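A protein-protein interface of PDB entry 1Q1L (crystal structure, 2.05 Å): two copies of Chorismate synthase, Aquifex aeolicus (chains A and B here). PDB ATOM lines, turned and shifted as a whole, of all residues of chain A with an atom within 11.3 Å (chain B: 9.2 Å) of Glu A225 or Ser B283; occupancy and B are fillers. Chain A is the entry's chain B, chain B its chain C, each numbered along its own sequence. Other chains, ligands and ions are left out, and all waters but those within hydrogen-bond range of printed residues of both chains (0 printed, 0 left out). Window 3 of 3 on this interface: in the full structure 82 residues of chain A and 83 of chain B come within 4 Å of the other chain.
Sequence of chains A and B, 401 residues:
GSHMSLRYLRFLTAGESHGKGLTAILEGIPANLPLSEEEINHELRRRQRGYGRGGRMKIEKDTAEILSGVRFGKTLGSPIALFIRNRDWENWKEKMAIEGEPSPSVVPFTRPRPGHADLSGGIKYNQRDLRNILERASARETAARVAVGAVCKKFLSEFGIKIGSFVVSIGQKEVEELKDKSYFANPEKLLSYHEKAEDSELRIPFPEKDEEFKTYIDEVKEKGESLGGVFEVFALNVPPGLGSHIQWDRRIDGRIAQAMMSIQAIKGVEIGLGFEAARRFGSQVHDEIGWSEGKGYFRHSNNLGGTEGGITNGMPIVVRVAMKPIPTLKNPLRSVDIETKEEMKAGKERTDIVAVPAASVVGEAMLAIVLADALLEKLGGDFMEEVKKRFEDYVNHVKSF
Phe B281 touches Gln A172. Phe B281 touches Val A220. Gly B282 touches Glu A225 (N to OE2, 3.6 Å). Phe B281 touches Ser A226. CD2 of Phe B281 touches CD2 of Leu A227, 3.9 Å away. Pro A325 touches Ala B277 (CD to O, 3.1 Å). CG of Pro A325 touches O of Arg B280, 3.3 Å away. Pro A325 touches Phe B281 (CG to C, 3.9 Å). CA of Gly B282 touches CB of Pro A325, at 3.3 Å. His B286 touches Thr A328 (CB to O, 3.98 Å).
OE1 of Glu A225 is in hydrogen-bond range of OG of Ser B283. N of Gly B282 is in hydrogen-bond range of O of Ser A226. N of Ser B283 lies within hydrogen-bond range of O of Thr A328, at 2.7 Å. The backbone carbonyl oxygen (O) of Thr A328 lies close to the backbone carbonyl oxygen (O) of Gly B282, at 3.1 Å.
Of the printed residues of chain B, Glu A225 touches Phe B281 (3.3 Å), Gly B282 (3.6 Å) and Ser B283 (2.6 Å). Ser B283 touches just these residues of chain A: Glu A225 (2.6 Å) and Thr A328 (2.7 Å). Gly A224 touches none of the printed residues of chain B. Of the printed residues of chain A, Gly B282 touches Glu A225, Ser A226, Pro A325 and Thr A328. Val B285 touches just one residue of chain A: Pro A325. Of the printed residues of chain A, His B286 touches Thr A328 (3.98 Å). Of the printed residues of chain B, Thr A328 touches Gly B282, Ser B283 and His B286. Of the printed residues of chain B, Pro A325 touches Ala B277 (3.1 Å), Arg B280 (3.3 Å), Phe B281 (3.9 Å), Gly B282 (3.3 Å) and Val B285 (3.9 Å). Printed residues of chain B within 4 Å of Gln A172: Arg B280 (3.7 Å) and Phe B281 (3.7 Å). The nearest residue of chain B that does not touch Glu A225 is Gln B284 (5.1 Å). The nearest residue of chain A that does not touch Ser B283 is Ser A226 (4.7 Å). The nearest printed residue of chain A that does not touch Ala B277 is Lys A324 (4.3 Å).
No position is printed for both chains. Of the 17 pairs that touch across the chains among the printed residues, none has its exchanged pair printed and touching as well.
Printed residues of chain A that touch a printed residue of chain B: Gln A172, Val A220, Glu A225, Ser A226, Leu A227, Pro A325 and Thr A328. Hydrophobic or aromatic side chains of chain A that line the printed part of chain B: Val A220, Leu A227 and Pro A325. Along chain A the printed residues that touch a printed residue of chain B span positions 172 to 328. Of the 13 printed residues of chain B, 7 touch a printed residue of chain A. Hydrophobic or aromatic side chains of chain B that line the printed part of chain A: Phe B281, Val B285 and His B286.
The side-chain hydroxyl of Tyr A216 sits at hydrogen-bond distance from the backbone NH of Gln A172, 2.9 Å away. O of Val A220 sits close to N of Glu A225 (3.2 Å). The backbone NH of Phe B281 is in hydrogen-bond range of the side-chain amide oxygen of Gln B284. The side-chain amide oxygen of Asn B303 lies close to the backbone carbonyl oxygen of Val B285, at 2.6 Å. The side-chain hydroxyl (OG) of Ser B301 is in hydrogen-bond range of the backbone carbonyl oxygen (O) of His B286, 3.4 Å away.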
ATOM      1  N   ILE A 170      22.372  24.264   3.800  1.00  0.00           N
ATOM      2  CA  ILE A 170      22.204  25.466   4.604  1.00  0.00           C
ATOM      3  C   ILE A 170      20.698  25.633   4.735  1.00  0.00           C
ATOM      4  O   ILE A 170      19.984  25.689   3.733  1.00  0.00           O
ATOM      5  CB  ILE A 170      22.796  26.708   3.912  1.00  0.00           C
ATOM      6  CG1 ILE A 170      24.278  26.476   3.619  1.00  0.00           C
ATOM      7  CG2 ILE A 170      22.611  27.934   4.796  1.00  0.00           C
ATOM      8  CD1 ILE A 170      25.002  27.687   3.057  1.00  0.00           C
ATOM      9  N   GLY A 171      20.212  25.693   5.971  1.00  0.00           N
ATOM     10  CA  GLY A 171      18.785  25.819   6.174  1.00  0.00           C
ATOM     11  C   GLY A 171      18.094  24.590   5.615  1.00  0.00           C
ATOM     12  O   GLY A 171      18.549  23.462   5.823  1.00  0.00           O
ATOM     13  N   GLN A 172      17.001  24.807   4.889  1.00  0.00           N
ATOM     14  CA  GLN A 172      16.235  23.718   4.296  1.00  0.00           C
ATOM     15  C   GLN A 172      16.802  23.412   2.914  1.00  0.00           C
ATOM     16  O   GLN A 172      16.370  22.469   2.247  1.00  0.00           O
ATOM     17  CB  GLN A 172      14.767  24.133   4.148  1.00  0.00           C
ATOM     18  CG  GLN A 172      14.246  25.017   5.271  1.00  0.00           C
ATOM     19  CD  GLN A 172      14.001  24.256   6.557  1.00  0.00           C
ATOM     20  OE1 GLN A 172      13.730  24.854   7.602  1.00  0.00           O
ATOM     21  NE2 GLN A 172      14.083  22.931   6.489  1.00  0.00           N
ATOM     22  N   LYS A 214      22.520  32.403  -1.707  1.00  0.00           N
ATOM     23  CA  LYS A 214      22.547  33.757  -1.159  1.00  0.00           C
ATOM     24  C   LYS A 214      21.139  34.328  -1.024  1.00  0.00           C
ATOM     25  O   LYS A 214      20.783  34.881   0.017  1.00  0.00           O
ATOM     26  CB  LYS A 214      23.370  34.685  -2.052  1.00  0.00           C
ATOM     27  CG  LYS A 214      24.862  34.415  -2.065  1.00  0.00           C
ATOM     28  CD  LYS A 214      25.561  35.465  -2.911  1.00  0.00           C
ATOM     29  CE  LYS A 214      27.066  35.293  -2.912  1.00  0.00           C
ATOM     30  NZ  LYS A 214      27.718  36.363  -3.721  1.00  0.00           N
ATOM     31  N   THR A 215      20.339  34.195  -2.079  1.00  0.00           N
ATOM     32  CA  THR A 215      18.975  34.708  -2.060  1.00  0.00           C
ATOM     33  C   THR A 215      18.152  34.007  -0.987  1.00  0.00           C
ATOM     34  O   THR A 215      17.584  34.661  -0.112  1.00  0.00           O
ATOM     35  CB  THR A 215      18.279  34.527  -3.428  1.00  0.00           C
ATOM     36  OG1 THR A 215      18.101  33.132  -3.700  1.00  0.00           O
ATOM     37  CG2 THR A 215      19.119  35.156  -4.537  1.00  0.00           C
ATOM     38  N   TYR A 216      18.090  32.678  -1.055  1.00  0.00           N
ATOM     39  CA  TYR A 216      17.342  31.896  -0.073  1.00  0.00           C
ATOM     40  C   TYR A 216      17.683  32.374   1.329  1.00  0.00           C
ATOM     41  O   TYR A 216      16.799  32.615   2.150  1.00  0.00           O
ATOM     42  CB  TYR A 216      17.681  30.408  -0.191  1.00  0.00           C
ATOM     43  CG  TYR A 216      17.234  29.599   1.007  1.00  0.00           C
ATOM     44  CD1 TYR A 216      15.883  29.486   1.333  1.00  0.00           C
ATOM     45  CD2 TYR A 216      18.166  28.980   1.839  1.00  0.00           C
ATOM     46  CE1 TYR A 216      15.470  28.779   2.461  1.00  0.00           C
ATOM     47  CE2 TYR A 216      17.765  28.272   2.969  1.00  0.00           C
ATOM     48  CZ  TYR A 216      16.418  28.176   3.274  1.00  0.00           C
ATOM     49  OH  TYR A 216      16.021  27.487   4.396  1.00  0.00           O
ATOM     50  N   ILE A 217      18.979  32.504   1.592  1.00  0.00           N
ATOM     51  CA  ILE A 217      19.462  32.960   2.886  1.00  0.00           C
ATOM     52  C   ILE A 217      18.902  34.351   3.173  1.00  0.00           C
ATOM     53  O   ILE A 217      18.278  34.578   4.211  1.00  0.00           O
ATOM     54  CB  ILE A 217      21.006  33.009   2.907  1.00  0.00           C
ATOM     55  CG1 ILE A 217      21.569  31.597   2.715  1.00  0.00           C
ATOM     56  CG2 ILE A 217      21.500  33.604   4.214  1.00  0.00           C
ATOM     57  CD1 ILE A 217      23.083  31.535   2.655  1.00  0.00           C
ATOM     58  N   ASP A 218      19.117  35.271   2.238  1.00  0.00           N
ATOM     59  CA  ASP A 218      18.640  36.641   2.379  1.00  0.00           C
ATOM     60  C   ASP A 218      17.159  36.684   2.732  1.00  0.00           C
ATOM     61  O   ASP A 218      16.744  37.463   3.591  1.00  0.00           O
ATOM     62  CB  ASP A 218      18.894  37.422   1.087  1.00  0.00           C
ATOM     63  CG  ASP A 218      20.374  37.623   0.811  1.00  0.00           C
ATOM     64  OD1 ASP A 218      20.716  38.187  -0.250  1.00  0.00           O
ATOM     65  OD2 ASP A 218      21.200  37.221   1.658  1.00  0.00           O
ATOM     66  N   GLU A 219      16.363  35.849   2.070  1.00  0.00           N
ATOM     67  CA  GLU A 219      14.931  35.798   2.344  1.00  0.00           C
ATOM     68  C   GLU A 219      14.704  35.406   3.800  1.00  0.00           C
ATOM     69  O   GLU A 219      13.874  35.998   4.491  1.00  0.00           O
ATOM     70  CB  GLU A 219      14.242  34.791   1.419  1.00  0.00           C
ATOM     71  CG  GLU A 219      14.171  35.230  -0.035  1.00  0.00           C
ATOM     72  CD  GLU A 219      13.476  34.213  -0.924  1.00  0.00           C
ATOM     73  OE1 GLU A 219      14.013  33.094  -1.084  1.00  0.00           O
ATOM     74  OE2 GLU A 219      12.394  34.531  -1.460  1.00  0.00           O
ATOM     75  N   VAL A 220      15.449  34.406   4.262  1.00  0.00           N
ATOM     76  CA  VAL A 220      15.334  33.945   5.640  1.00  0.00           C
ATOM     77  C   VAL A 220      15.814  35.048   6.577  1.00  0.00           C
ATOM     78  O   VAL A 220      15.338  35.170   7.705  1.00  0.00           O
ATOM     79  CB  VAL A 220      16.172  32.669   5.873  1.00  0.00           C
ATOM     80  CG1 VAL A 220      16.056  32.220   7.321  1.00  0.00           C
ATOM     81  CG2 VAL A 220      15.696  31.564   4.941  1.00  0.00           C
ATOM     82  N   LYS A 221      16.759  35.854   6.097  1.00  0.00           N
ATOM     83  CA  LYS A 221      17.292  36.963   6.882  1.00  0.00           C
ATOM     84  C   LYS A 221      16.215  38.029   7.069  1.00  0.00           C
ATOM     85  O   LYS A 221      16.042  38.564   8.164  1.00  0.00           O
ATOM     86  CB  LYS A 221      18.496  37.591   6.176  1.00  0.00           C
ATOM     87  CG  LYS A 221      19.737  36.719   6.120  1.00  0.00           C
ATOM     88  CD  LYS A 221      20.832  37.397   5.306  1.00  0.00           C
ATOM     89  CE  LYS A 221      22.154  36.650   5.399  1.00  0.00           C
ATOM     90  NZ  LYS A 221      22.700  36.649   6.786  1.00  0.00           N
ATOM     91  N   GLU A 222      15.495  38.332   5.990  1.00  0.00           N
ATOM     92  CA  GLU A 222      14.436  39.336   6.017  1.00  0.00           C
ATOM     93  C   GLU A 222      13.485  39.140   7.189  1.00  0.00           C
ATOM     94  O   GLU A 222      13.245  40.067   7.964  1.00  0.00           O
ATOM     95  CB  GLU A 222      13.633  39.311   4.710  1.00  0.00           C
ATOM     96  CG  GLU A 222      14.405  39.784   3.484  1.00  0.00           C
ATOM     97  CD  GLU A 222      13.524  39.911   2.251  1.00  0.00           C
ATOM     98  OE1 GLU A 222      12.553  40.697   2.291  1.00  0.00           O
ATOM     99  OE2 GLU A 222      13.803  39.226   1.244  1.00  0.00           O
ATOM    100  N   LYS A 223      12.942  37.932   7.314  1.00  0.00           N
ATOM    101  CA  LYS A 223      12.015  37.631   8.397  1.00  0.00           C
ATOM    102  C   LYS A 223      12.750  37.342   9.703  1.00  0.00           C
ATOM    103  O   LYS A 223      12.302  36.531  10.516  1.00  0.00           O
ATOM    104  CB  LYS A 223      11.115  36.453   8.010  1.00  0.00           C
ATOM    105  CG  LYS A 223      11.853  35.196   7.582  1.00  0.00           C
ATOM    106  CD  LYS A 223      10.892  34.185   6.964  1.00  0.00           C
ATOM    107  CE  LYS A 223       9.779  33.801   7.929  1.00  0.00           C
ATOM    108  NZ  LYS A 223       8.768  32.910   7.295  1.00  0.00           N
ATOM    109  N   GLY A 224      13.878  38.025   9.890  1.00  0.00           N
ATOM    110  CA  GLY A 224      14.678  37.871  11.094  1.00  0.00           C
ATOM    111  C   GLY A 224      14.884  36.441  11.554  1.00  0.00           C
ATOM    112  O   GLY A 224      14.344  36.026  12.578  1.00  0.00           O
ATOM    113  N   GLU A 225      15.671  35.683  10.799  1.00  0.00           N
ATOM    114  CA  GLU A 225      15.943  34.296  11.148  1.00  0.00           C
ATOM    115  C   GLU A 225      17.420  33.952  11.017  1.00  0.00           C
ATOM    116  O   GLU A 225      18.185  34.666  10.367  1.00  0.00           O
ATOM    117  CB  GLU A 225      15.119  33.356  10.266  1.00  0.00           C
ATOM    118  CG  GLU A 225      13.655  33.249  10.654  1.00  0.00           C
ATOM    119  CD  GLU A 225      13.447  32.503  11.960  1.00  0.00           C
ATOM    120  OE1 GLU A 225      12.280  32.374  12.387  1.00  0.00           O
ATOM    121  OE2 GLU A 225      14.443  32.044  12.559  1.00  0.00           O
ATOM    122  N   SER A 226      17.809  32.853  11.650  1.00  0.00           N
ATOM    123  CA  SER A 226      19.184  32.379  11.612  1.00  0.00           C
ATOM    124  C   SER A 226      19.150  30.963  11.052  1.00  0.00           C
ATOM    125  O   SER A 226      18.146  30.261  11.189  1.00  0.00           O
ATOM    126  CB  SER A 226      19.785  32.368  13.019  1.00  0.00           C
ATOM    127  OG  SER A 226      19.094  31.460  13.862  1.00  0.00           O
ATOM    128  N   LEU A 227      20.240  30.539  10.426  1.00  0.00           N
ATOM    129  CA  LEU A 227      20.283  29.205   9.846  1.00  0.00           C
ATOM    130  C   LEU A 227      21.474  28.368  10.274  1.00  0.00           C
ATOM    131  O   LEU A 227      22.546  28.886  10.573  1.00  0.00           O
ATOM    132  CB  LEU A 227      20.268  29.292   8.316  1.00  0.00           C
ATOM    133  CG  LEU A 227      18.982  29.796   7.658  1.00  0.00           C
ATOM    134  CD1 LEU A 227      19.189  29.888   6.153  1.00  0.00           C
ATOM    135  CD2 LEU A 227      17.824  28.851   7.989  1.00  0.00           C
ATOM    136  N   GLY A 228      21.258  27.060  10.302  1.00  0.00           N
ATOM    137  CA  GLY A 228      22.315  26.135  10.648  1.00  0.00           C
ATOM    138  C   GLY A 228      22.728  25.472   9.352  1.00  0.00           C
ATOM    139  O   GLY A 228      22.302  25.898   8.280  1.00  0.00           O
ATOM    140  N   MET A 323      25.573  21.550  12.233  1.00  0.00           N
ATOM    141  CA  MET A 323      25.665  22.760  13.042  1.00  0.00           C
ATOM    142  C   MET A 323      24.301  23.428  13.187  1.00  0.00           C
ATOM    143  O   MET A 323      23.650  23.744  12.191  1.00  0.00           O
ATOM    144  CB  MET A 323      26.631  23.753  12.411  1.00  0.00           C
ATOM    145  CG  MET A 323      26.832  24.992  13.248  1.00  0.00           C
ATOM    146  SD  MET A 323      27.638  26.416  12.260  1.00  0.00           S
ATOM    147  CE  MET A 323      26.007  27.355  11.791  1.00  0.00           C
ATOM    148  N   LYS A 324      23.884  23.653  14.431  1.00  0.00           N
ATOM    149  CA  LYS A 324      22.598  24.281  14.710  1.00  0.00           C
ATOM    150  C   LYS A 324      22.629  25.764  14.357  1.00  0.00           C
ATOM    151  O   LYS A 324      23.700  26.356  14.201  1.00  0.00           O
ATOM    152  CB  LYS A 324      22.249  24.144  16.192  1.00  0.00           C
ATOM    153  CG  LYS A 324      23.122  25.007  17.084  1.00  0.00           C
ATOM    154  CD  LYS A 324      22.558  25.139  18.484  1.00  0.00           C
ATOM    155  CE  LYS A 324      23.342  26.180  19.264  1.00  0.00           C
ATOM    156  NZ  LYS A 324      22.736  26.477  20.584  1.00  0.00           N
ATOM    157  N   PRO A 325      21.444  26.382  14.229  1.00  0.00           N
ATOM    158  CA  PRO A 325      21.305  27.805  13.901  1.00  0.00           C
ATOM    159  C   PRO A 325      21.931  28.666  14.991  1.00  0.00           C
ATOM    160  O   PRO A 325      21.679  28.450  16.177  1.00  0.00           O
ATOM    161  CB  PRO A 325      19.791  28.000  13.839  1.00  0.00           C
ATOM    162  CG  PRO A 325      19.289  26.660  13.425  1.00  0.00           C
ATOM    163  CD  PRO A 325      20.124  25.728  14.261  1.00  0.00           C
ATOM    164  N   ILE A 326      22.737  29.641  14.589  1.00  0.00           N
ATOM    165  CA  ILE A 326      23.389  30.533  15.537  1.00  0.00           C
ATOM    166  C   ILE A 326      22.833  31.946  15.384  1.00  0.00           C
ATOM    167  O   ILE A 326      23.004  32.573  14.338  1.00  0.00           O
ATOM    168  CB  ILE A 326      24.912  30.592  15.296  1.00  0.00           C
ATOM    169  CG1 ILE A 326      25.500  29.180  15.291  1.00  0.00           C
ATOM    170  CG2 ILE A 326      25.576  31.434  16.377  1.00  0.00           C
ATOM    171  CD1 ILE A 326      26.970  29.140  14.923  1.00  0.00           C
ATOM    172  N   PRO A 327      22.177  32.473  16.430  1.00  0.00           N
ATOM    173  CA  PRO A 327      21.940  31.807  17.713  1.00  0.00           C
ATOM    174  C   PRO A 327      20.469  31.456  17.953  1.00  0.00           C
ATOM    175  O   PRO A 327      20.072  30.297  17.847  1.00  0.00           O
ATOM    176  CB  PRO A 327      22.451  32.835  18.706  1.00  0.00           C
ATOM    177  CG  PRO A 327      21.930  34.119  18.101  1.00  0.00           C
ATOM    178  CD  PRO A 327      22.093  33.937  16.585  1.00  0.00           C
ATOM    179  N   THR A 328      19.673  32.471  18.283  1.00  0.00           N
ATOM    180  CA  THR A 328      18.249  32.291  18.554  1.00  0.00           C
ATOM    181  C   THR A 328      17.537  31.589  17.402  1.00  0.00           C
ATOM    182  O   THR A 328      16.341  31.792  17.183  1.00  0.00           O
ATOM    183  CB  THR A 328      17.559  33.653  18.808  1.00  0.00           C
ATOM    184  OG1 THR A 328      16.187  33.437  19.168  1.00  0.00           O
ATOM    185  CG2 THR A 328      17.622  34.525  17.557  1.00  0.00           C
ATOM    186  N   VAL A 354      24.462  32.519   9.165  1.00  0.00           N
ATOM    187  CA  VAL A 354      25.089  31.367   8.524  1.00  0.00           C
ATOM    188  C   VAL A 354      26.593  31.319   8.793  1.00  0.00           C
ATOM    189  O   VAL A 354      27.369  32.050   8.177  1.00  0.00           O
ATOM    190  CB  VAL A 354      24.863  31.389   6.997  1.00  0.00           C
ATOM    191  CG1 VAL A 354      25.456  30.136   6.363  1.00  0.00           C
ATOM    192  CG2 VAL A 354      23.375  31.487   6.695  1.00  0.00           C
ATOM    193  N   ALA A 355      26.999  30.452   9.712  1.00  0.00           N
ATOM    194  CA  ALA A 355      28.410  30.310  10.051  1.00  0.00           C
ATOM    195  C   ALA A 355      28.906  28.922   9.671  1.00  0.00           C
ATOM    196  O   ALA A 355      30.038  28.552   9.980  1.00  0.00           O
ATOM    197  CB  ALA A 355      28.618  30.551  11.545  1.00  0.00           C
ATOM    198  N   LEU B 273      17.966  17.527  18.845  1.00  0.00           N
ATOM    199  CA  LEU B 273      17.464  17.360  17.480  1.00  0.00           C
ATOM    200  C   LEU B 273      18.508  16.846  16.497  1.00  0.00           C
ATOM    201  O   LEU B 273      18.167  16.173  15.522  1.00  0.00           O
ATOM    202  CB  LEU B 273      16.900  18.681  16.948  1.00  0.00           C
ATOM    203  CG  LEU B 273      15.455  19.055  17.285  1.00  0.00           C
ATOM    204  CD1 LEU B 273      15.085  20.312  16.511  1.00  0.00           C
ATOM    205  CD2 LEU B 273      14.512  17.919  16.910  1.00  0.00           C
ATOM    206  N   ALA B 277      17.987  19.839  13.614  1.00  0.00           N
ATOM    207  CA  ALA B 277      18.177  21.202  14.084  1.00  0.00           C
ATOM    208  C   ALA B 277      18.976  22.001  13.067  1.00  0.00           C
ATOM    209  O   ALA B 277      18.845  23.224  12.980  1.00  0.00           O
ATOM    210  CB  ALA B 277      18.895  21.197  15.425  1.00  0.00           C
ATOM    211  N   ARG B 280      16.340  23.378  10.441  1.00  0.00           N
ATOM    212  CA  ARG B 280      15.344  24.360  10.870  1.00  0.00           C
ATOM    213  C   ARG B 280      15.871  25.772  11.101  1.00  0.00           C
ATOM    214  O   ARG B 280      17.075  26.012  11.046  1.00  0.00           O
ATOM    215  CB  ARG B 280      14.648  23.860  12.137  1.00  0.00           C
ATOM    216  CG  ARG B 280      14.085  22.454  12.001  1.00  0.00           C
ATOM    217  CD  ARG B 280      13.292  22.038  13.227  1.00  0.00           C
ATOM    218  NE  ARG B 280      12.958  20.617  13.195  1.00  0.00           N
ATOM    219  CZ  ARG B 280      12.315  19.976  14.167  1.00  0.00           C
ATOM    220  NH1 ARG B 280      11.926  20.628  15.256  1.00  0.00           N
ATOM    221  NH2 ARG B 280      12.067  18.674  14.058  1.00  0.00           N
ATOM    222  N   PHE B 281      14.952  26.705  11.353  1.00  0.00           N
ATOM    223  CA  PHE B 281      15.320  28.095  11.603  1.00  0.00           C
ATOM    224  C   PHE B 281      15.718  28.260  13.063  1.00  0.00           C
ATOM    225  O   PHE B 281      15.278  27.497  13.925  1.00  0.00           O
ATOM    226  CB  PHE B 281      14.151  29.045  11.312  1.00  0.00           C
ATOM    227  CG  PHE B 281      13.611  28.953   9.911  1.00  0.00           C
ATOM    228  CD1 PHE B 281      12.552  28.099   9.613  1.00  0.00           C
ATOM    229  CD2 PHE B 281      14.149  29.732   8.892  1.00  0.00           C
ATOM    230  CE1 PHE B 281      12.033  28.023   8.320  1.00  0.00           C
ATOM    231  CE2 PHE B 281      13.640  29.665   7.594  1.00  0.00           C
ATOM    232  CZ  PHE B 281      12.580  28.808   7.308  1.00  0.00           C
ATOM    233  N   GLY B 282      16.542  29.266  13.334  1.00  0.00           N
ATOM    234  CA  GLY B 282      16.975  29.514  14.695  1.00  0.00           C
ATOM    235  C   GLY B 282      15.838  29.508  15.701  1.00  0.00           C
ATOM    236  O   GLY B 282      15.852  28.736  16.661  1.00  0.00           O
ATOM    237  N   SER B 283      14.845  30.364  15.481  1.00  0.00           N
ATOM    238  CA  SER B 283      13.707  30.460  16.389  1.00  0.00           C
ATOM    239  C   SER B 283      13.017  29.121  16.636  1.00  0.00           C
ATOM    240  O   SER B 283      12.377  28.929  17.670  1.00  0.00           O
ATOM    241  CB  SER B 283      12.687  31.469  15.852  1.00  0.00           C
ATOM    242  OG  SER B 283      12.122  31.028  14.630  1.00  0.00           O
ATOM    243  N   GLN B 284      13.155  28.193  15.694  1.00  0.00           N
ATOM    244  CA  GLN B 284      12.521  26.886  15.821  1.00  0.00           C
ATOM    245  C   GLN B 284      13.228  25.926  16.778  1.00  0.00           C
ATOM    246  O   GLN B 284      12.571  25.175  17.495  1.00  0.00           O
ATOM    247  CB  GLN B 284      12.396  26.225  14.444  1.00  0.00           C
ATOM    248  CG  GLN B 284      11.514  26.981  13.459  1.00  0.00           C
ATOM    249  CD  GLN B 284      11.325  26.232  12.150  1.00  0.00           C
ATOM    250  OE1 GLN B 284      12.294  25.908  11.462  1.00  0.00           O
ATOM    251  NE2 GLN B 284      10.071  25.951  11.801  1.00  0.00           N
ATOM    252  N   VAL B 285      14.556  25.942  16.791  1.00  0.00           N
ATOM    253  CA  VAL B 285      15.298  25.044  17.672  1.00  0.00           C
ATOM    254  C   VAL B 285      15.513  25.642  19.064  1.00  0.00           C
ATOM    255  O   VAL B 285      15.473  24.928  20.065  1.00  0.00           O
ATOM    256  CB  VAL B 285      16.685  24.676  17.076  1.00  0.00           C
ATOM    257  CG1 VAL B 285      16.542  24.335  15.604  1.00  0.00           C
ATOM    258  CG2 VAL B 285      17.672  25.819  17.272  1.00  0.00           C
ATOM    259  N   HIS B 286      15.730  26.954  19.111  1.00  0.00           N
ATOM    260  CA  HIS B 286      15.976  27.675  20.359  1.00  0.00           C
ATOM    261  C   HIS B 286      15.105  27.241  21.534  1.00  0.00           C
ATOM    262  O   HIS B 286      13.878  27.198  21.435  1.00  0.00           O
ATOM    263  CB  HIS B 286      15.799  29.180  20.132  1.00  0.00           C
ATOM    264  CG  HIS B 286      16.023  30.008  21.360  1.00  0.00           C
ATOM    265  ND1 HIS B 286      17.237  30.060  22.012  1.00  0.00           N
ATOM    266  CD2 HIS B 286      15.188  30.815  22.057  1.00  0.00           C
ATOM    267  CE1 HIS B 286      17.139  30.861  23.059  1.00  0.00           C
ATOM    268  NE2 HIS B 286      15.906  31.332  23.107  1.00  0.00           N
ATOM    269  N   ASP B 287      15.752  26.908  22.647  1.00  0.00           N
ATOM    270  CA  ASP B 287      15.031  26.515  23.849  1.00  0.00           C
ATOM    271  C   ASP B 287      14.926  27.768  24.717  1.00  0.00           C
ATOM    272  O   ASP B 287      15.898  28.185  25.348  1.00  0.00           O
ATOM    273  CB  ASP B 287      15.779  25.414  24.612  1.00  0.00           C
ATOM    274  CG  ASP B 287      15.867  24.110  23.831  1.00  0.00           C
ATOM    275  OD1 ASP B 287      14.856  23.707  23.213  1.00  0.00           O
ATOM    276  OD2 ASP B 287      16.944  23.475  23.851  1.00  0.00           O
ATOM    277  N   GLU B 288      13.742  28.369  24.735  1.00  0.00           N
ATOM    278  CA  GLU B 288      13.506  29.584  25.506  1.00  0.00           C
ATOM    279  C   GLU B 288      13.742  29.376  27.000  1.00  0.00           C
ATOM    280  O   GLU B 288      13.253  28.417  27.590  1.00  0.00           O
ATOM    281  CB  GLU B 288      12.074  30.079  25.276  1.00  0.00           C
ATOM    282  CG  GLU B 288      11.759  31.400  25.962  1.00  0.00           C
ATOM    283  CD  GLU B 288      10.343  31.882  25.692  1.00  0.00           C
ATOM    284  OE1 GLU B 288      10.009  33.003  26.120  1.00  0.00           O
ATOM    285  OE2 GLU B 288       9.562  31.142  25.055  1.00  0.00           O
ATOM    286  N   SER B 301      11.600  24.205  25.937  1.00  0.00           N
ATOM    287  CA  SER B 301      11.724  23.111  24.976  1.00  0.00           C
ATOM    288  C   SER B 301      13.131  22.550  25.173  1.00  0.00           C
ATOM    289  O   SER B 301      13.963  23.194  25.810  1.00  0.00           O
ATOM    290  CB  SER B 301      11.532  23.607  23.535  1.00  0.00           C
ATOM    291  OG  SER B 301      12.414  24.670  23.202  1.00  0.00           O
ATOM    292  N   ASN B 303      15.348  21.084  22.472  1.00  0.00           N
ATOM    293  CA  ASN B 303      15.891  20.678  21.182  1.00  0.00           C
ATOM    294  C   ASN B 303      17.408  20.503  21.300  1.00  0.00           C
ATOM    295  O   ASN B 303      18.029  19.824  20.484  1.00  0.00           O
ATOM    296  CB  ASN B 303      15.588  21.734  20.118  1.00  0.00           C
ATOM    297  CG  ASN B 303      14.100  21.926  19.892  1.00  0.00           C
ATOM    298  OD1 ASN B 303      13.625  23.054  19.791  1.00  0.00           O
ATOM    299  ND2 ASN B 303      13.359  20.825  19.806  1.00  0.00           N
